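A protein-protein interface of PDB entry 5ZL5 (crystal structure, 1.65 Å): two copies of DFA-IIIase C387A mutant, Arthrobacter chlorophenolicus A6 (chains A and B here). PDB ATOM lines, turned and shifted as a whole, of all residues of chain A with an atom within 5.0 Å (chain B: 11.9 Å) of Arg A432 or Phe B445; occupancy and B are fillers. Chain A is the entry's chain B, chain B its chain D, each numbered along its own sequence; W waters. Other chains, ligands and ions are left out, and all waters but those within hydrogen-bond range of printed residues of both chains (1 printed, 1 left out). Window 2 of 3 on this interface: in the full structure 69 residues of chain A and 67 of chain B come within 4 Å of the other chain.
Water W1 lies within hydrogen-bond range of the backbone carbonyl oxygen (O) of Thr B442 (2.7 Å), the backbone carbonyl oxygen (O) of Gly B444 (2.9 Å) and the backbone NH (N) of Ile A437 (3.0 Å).
No position is printed for both chains.
Among the printed residues, merely in contact across the chains: Ala A433 with Val B443 (3.3 Å), Val A434 with Val B443 (3.4 Å), Arg A432 with Phe B445 (3.6 Å), Asn A435 with Val B443 (3.7 Å), Ala A433 with Phe B445 (3.7 Å) and Ala A433 with Gly B444 (3.7 Å).
Of the 10 printed residues of chain A, 4 touch a printed residue of chain B. Hydrophobic or aromatic side chains of chain B within 4 Å of the printed part of chain A: Val B443 and Phe B445. Among the printed residues, 8 pairs touch across the chains. Among the printed residues, no Asp or Glu carboxylate lies within 4 Å of a Lys or Arg side-chain nitrogen of the other chain.
The backbone carbonyl oxygen (O) of Arg A432 lies close to the backbone NH (N) of Gly B444, at 3.4 Å. The backbone carbonyl oxygen of Asn A435 lies within hydrogen-bond range of the backbone NH of Gly B444 (3.1 Å).
The side-chain carboxylate (OD1) of Asp A425 lies within salt-bridge range of the guanidinium group (NH2) of Arg A432, 3.0 Å away. The backbone carbonyl oxygen (O) of Val A428 lies within hydrogen-bond range of the guanidinium group (NH1) of Arg A432 (2.7 Å). The guanidinium group (NH1) of Arg A432 sits at hydrogen-bond distance from the backbone carbonyl oxygen (O) of Ala A430, 3.0 Å away. The backbone NH (N) of Ala A433 lies within hydrogen-bond range of the side-chain carboxylate (OD1) of Asp A431. O of Asp A431 lies within hydrogen-bond range of ND2 of Asn A435.
No residue of chain B comes within 4 Å of Val A428. No residue of chain B comes within 4 Å of Val A429. No residue of chain B comes within 4 Å of Ala A430. No residue of chain B comes within 4 Å of Asp A431. Arg A432 touches two residues of chain B. Ala A433 touches just these residues of chain B: Val B443 (3.3 Å), Gly B444 (3.7 Å) and Phe B445 (3.7 Å). Of the printed residues of chain B, Val A434 touches Val B443. No residue of chain B comes within 4 Å of Ile A437. Pro B441 touches none of the printed residues of chain A. Thr B442 touches none of the printed residues of chain A. Printed residues of chain A within 4 Å of Val B443: Ala A433 (3.3 Å), Val A434 (3.4 Å) and Asn A435 (3.7 Å). Printed residues of chain A within 4 Å of Gly B444: Arg A432, Ala A433 and Asn A435. The nearest printed residue of chain A that does not touch Phe B445 is Asp A431 (5.6 Å). The nearest printed residue of chain A that does not touch Val B443 is Arg A432 (4.7 Å).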
ATOM      1  N   ASP A 425      24.457 -17.266 -10.197  1.00  0.00           N
ATOM      2  CA  ASP A 425      24.005 -16.049 -10.868  1.00  0.00           C
ATOM      3  C   ASP A 425      25.054 -15.470 -11.808  1.00  0.00           C
ATOM      4  O   ASP A 425      24.709 -15.076 -12.921  1.00  0.00           O
ATOM      5  CB  ASP A 425      23.559 -14.970  -9.871  1.00  0.00           C
ATOM      6  CG  ASP A 425      22.102 -15.063  -9.525  1.00  0.00           C
ATOM      7  OD1 ASP A 425      21.259 -15.399 -10.394  1.00  0.00           O
ATOM      8  OD2 ASP A 425      21.790 -14.792  -8.352  1.00  0.00           O
ATOM      9  N   VAL A 428      25.152 -17.352 -15.160  1.00  0.00           N
ATOM     10  CA  VAL A 428      23.975 -17.306 -16.010  1.00  0.00           C
ATOM     11  C   VAL A 428      23.840 -15.880 -16.492  1.00  0.00           C
ATOM     12  O   VAL A 428      23.547 -14.979 -15.702  1.00  0.00           O
ATOM     13  CB  VAL A 428      22.699 -17.768 -15.273  1.00  0.00           C
ATOM     14  CG1 VAL A 428      21.461 -17.619 -16.164  1.00  0.00           C
ATOM     15  CG2 VAL A 428      22.838 -19.224 -14.828  1.00  0.00           C
ATOM     16  N   VAL A 429      24.095 -15.674 -17.777  1.00  0.00           N
ATOM     17  CA  VAL A 429      24.041 -14.342 -18.394  1.00  0.00           C
ATOM     18  C   VAL A 429      22.713 -14.317 -19.142  1.00  0.00           C
ATOM     19  O   VAL A 429      22.528 -15.018 -20.140  1.00  0.00           O
ATOM     20  CB  VAL A 429      25.262 -14.096 -19.295  1.00  0.00           C
ATOM     21  CG1 VAL A 429      25.146 -12.767 -20.042  1.00  0.00           C
ATOM     22  CG2 VAL A 429      26.529 -14.105 -18.457  1.00  0.00           C
ATOM     23  N   ALA A 430      21.762 -13.558 -18.612  1.00  0.00           N
ATOM     24  CA  ALA A 430      20.400 -13.561 -19.118  1.00  0.00           C
ATOM     25  C   ALA A 430      19.612 -12.391 -18.521  1.00  0.00           C
ATOM     26  O   ALA A 430      19.832 -11.991 -17.380  1.00  0.00           O
ATOM     27  CB  ALA A 430      19.697 -14.873 -18.761  1.00  0.00           C
ATOM     28  N   ASP A 431      18.645 -11.905 -19.295  1.00  0.00           N
ATOM     29  CA  ASP A 431      17.723 -10.872 -18.838  1.00  0.00           C
ATOM     30  C   ASP A 431      16.744 -11.462 -17.799  1.00  0.00           C
ATOM     31  O   ASP A 431      15.873 -12.290 -18.134  1.00  0.00           O
ATOM     32  CB  ASP A 431      16.997 -10.334 -20.072  1.00  0.00           C
ATOM     33  CG  ASP A 431      16.046  -9.189 -19.764  1.00  0.00           C
ATOM     34  OD1 ASP A 431      15.858  -8.832 -18.588  1.00  0.00           O
ATOM     35  OD2 ASP A 431      15.483  -8.667 -20.739  1.00  0.00           O
ATOM     36  N   ARG A 432      16.907 -11.065 -16.535  1.00  0.00           N
ATOM     37  CA  ARG A 432      16.063 -11.581 -15.457  1.00  0.00           C
ATOM     38  C   ARG A 432      14.616 -11.117 -15.557  1.00  0.00           C
ATOM     39  O   ARG A 432      13.749 -11.747 -14.993  1.00  0.00           O
ATOM     40  CB  ARG A 432      16.610 -11.244 -14.061  1.00  0.00           C
ATOM     41  CG  ARG A 432      17.506 -12.318 -13.449  1.00  0.00           C
ATOM     42  CD  ARG A 432      18.809 -12.466 -14.201  1.00  0.00           C
ATOM     43  NE  ARG A 432      19.740 -13.354 -13.481  1.00  0.00           N
ATOM     44  CZ  ARG A 432      20.876 -13.829 -13.980  1.00  0.00           C
ATOM     45  NH1 ARG A 432      21.264 -13.525 -15.225  1.00  0.00           N
ATOM     46  NH2 ARG A 432      21.645 -14.610 -13.229  1.00  0.00           N
ATOM     47  N   ALA A 433      14.359 -10.021 -16.268  1.00  0.00           N
ATOM     48  CA  ALA A 433      12.989  -9.500 -16.378  1.00  0.00           C
ATOM     49  C   ALA A 433      12.061 -10.431 -17.159  1.00  0.00           C
ATOM     50  O   ALA A 433      10.865 -10.483 -16.885  1.00  0.00           O
ATOM     51  CB  ALA A 433      12.998  -8.116 -17.002  1.00  0.00           C
ATOM     52  N   VAL A 434      12.622 -11.159 -18.122  1.00  0.00           N
ATOM     53  CA  VAL A 434      11.835 -11.869 -19.137  1.00  0.00           C
ATOM     54  C   VAL A 434      12.059 -13.383 -19.164  1.00  0.00           C
ATOM     55  O   VAL A 434      11.468 -14.070 -19.969  1.00  0.00           O
ATOM     56  CB  VAL A 434      12.065 -11.272 -20.547  1.00  0.00           C
ATOM     57  CG1 VAL A 434      11.790  -9.786 -20.518  1.00  0.00           C
ATOM     58  CG2 VAL A 434      13.464 -11.564 -21.065  1.00  0.00           C
ATOM     59  N   ASN A 435      12.891 -13.890 -18.266  1.00  0.00           N
ATOM     60  CA  ASN A 435      13.131 -15.322 -18.115  1.00  0.00           C
ATOM     61  C   ASN A 435      12.949 -15.625 -16.633  1.00  0.00           C
ATOM     62  O   ASN A 435      13.024 -14.703 -15.804  1.00  0.00           O
ATOM     63  CB  ASN A 435      14.565 -15.679 -18.528  1.00  0.00           C
ATOM     64  CG  ASN A 435      14.870 -15.367 -19.982  1.00  0.00           C
ATOM     65  OD1 ASN A 435      14.505 -16.123 -20.884  1.00  0.00           O
ATOM     66  ND2 ASN A 435      15.602 -14.290 -20.210  1.00  0.00           N
ATOM     67  N   ILE A 437      14.625 -17.448 -13.662  1.00  0.00           N
ATOM     68  CA  ILE A 437      15.993 -17.889 -13.328  1.00  0.00           C
ATOM     69  C   ILE A 437      16.099 -18.276 -11.854  1.00  0.00           C
ATOM     70  O   ILE A 437      15.745 -17.481 -10.995  1.00  0.00           O
ATOM     71  CB  ILE A 437      17.008 -16.794 -13.692  1.00  0.00           C
ATOM     72  CG1 ILE A 437      16.989 -16.586 -15.224  1.00  0.00           C
ATOM     73  CG2 ILE A 437      18.414 -17.177 -13.258  1.00  0.00           C
ATOM     74  CD1 ILE A 437      17.726 -15.362 -15.701  1.00  0.00           C
ATOM     75  N   THR B 440       7.328 -24.270 -10.180  1.00  0.00           N
ATOM     76  CA  THR B 440       8.405 -23.775 -11.023  1.00  0.00           C
ATOM     77  C   THR B 440       8.521 -22.250 -10.834  1.00  0.00           C
ATOM     78  O   THR B 440       7.498 -21.558 -10.807  1.00  0.00           O
ATOM     79  CB  THR B 440       8.132 -24.104 -12.497  1.00  0.00           C
ATOM     80  OG1 THR B 440       7.904 -25.517 -12.634  1.00  0.00           O
ATOM     81  CG2 THR B 440       9.298 -23.660 -13.378  1.00  0.00           C
ATOM     82  N   PRO B 441       9.744 -21.715 -10.659  1.00  0.00           N
ATOM     83  CA  PRO B 441       9.880 -20.258 -10.545  1.00  0.00           C
ATOM     84  C   PRO B 441       9.243 -19.490 -11.709  1.00  0.00           C
ATOM     85  O   PRO B 441       9.301 -19.947 -12.852  1.00  0.00           O
ATOM     86  CB  PRO B 441      11.397 -20.060 -10.545  1.00  0.00           C
ATOM     87  CG  PRO B 441      11.903 -21.282  -9.866  1.00  0.00           C
ATOM     88  CD  PRO B 441      11.016 -22.396 -10.335  1.00  0.00           C
ATOM     89  N   THR B 442       8.652 -18.341 -11.400  1.00  0.00           N
ATOM     90  CA  THR B 442       7.998 -17.482 -12.392  1.00  0.00           C
ATOM     91  C   THR B 442       9.024 -16.595 -13.080  1.00  0.00           C
ATOM     92  O   THR B 442      10.099 -16.334 -12.552  1.00  0.00           O
ATOM     93  CB  THR B 442       6.966 -16.553 -11.732  1.00  0.00           C
ATOM     94  OG1 THR B 442       7.612 -15.786 -10.710  1.00  0.00           O
ATOM     95  CG2 THR B 442       5.834 -17.343 -11.108  1.00  0.00           C
ATOM     96  N   VAL B 443       8.666 -16.116 -14.260  1.00  0.00           N
ATOM     97  CA  VAL B 443       9.473 -15.123 -14.958  1.00  0.00           C
ATOM     98  C   VAL B 443       9.614 -13.886 -14.073  1.00  0.00           C
ATOM     99  O   VAL B 443       8.653 -13.487 -13.393  1.00  0.00           O
ATOM    100  CB  VAL B 443       8.815 -14.721 -16.302  1.00  0.00           C
ATOM    101  CG1 VAL B 443       9.505 -13.514 -16.912  1.00  0.00           C
ATOM    102  CG2 VAL B 443       8.837 -15.888 -17.279  1.00  0.00           C
ATOM    103  N   GLY B 444      10.806 -13.287 -14.081  1.00  0.00           N
ATOM    104  CA  GLY B 444      11.014 -11.970 -13.488  1.00  0.00           C
ATOM    105  C   GLY B 444      11.596 -12.001 -12.097  1.00  0.00           C
ATOM    106  O   GLY B 444      12.312 -12.942 -11.723  1.00  0.00           O
ATOM    107  N   PHE B 445      11.291 -10.967 -11.315  1.00  0.00           N
ATOM    108  CA  PHE B 445      11.895 -10.780  -9.985  1.00  0.00           C
ATOM    109  C   PHE B 445      10.916 -11.203  -8.908  1.00  0.00           C
ATOM    110  O   PHE B 445      11.313 -11.895  -7.993  1.00  0.00           O
ATOM    111  CB  PHE B 445      12.333  -9.328  -9.798  1.00  0.00           C
ATOM    112  CG  PHE B 445      13.021  -8.768 -11.004  1.00  0.00           C
ATOM    113  CD1 PHE B 445      14.377  -9.016 -11.234  1.00  0.00           C
ATOM    114  CD2 PHE B 445      12.293  -8.051 -11.966  1.00  0.00           C
ATOM    115  CE1 PHE B 445      14.993  -8.524 -12.376  1.00  0.00           C
ATOM    116  CE2 PHE B 445      12.913  -7.552 -13.093  1.00  0.00           C
ATOM    117  CZ  PHE B 445      14.258  -7.795 -13.303  1.00  0.00           C
HETATM  118  O   HOH W   1      12.686 -15.798 -12.054  1.00  0.00           O
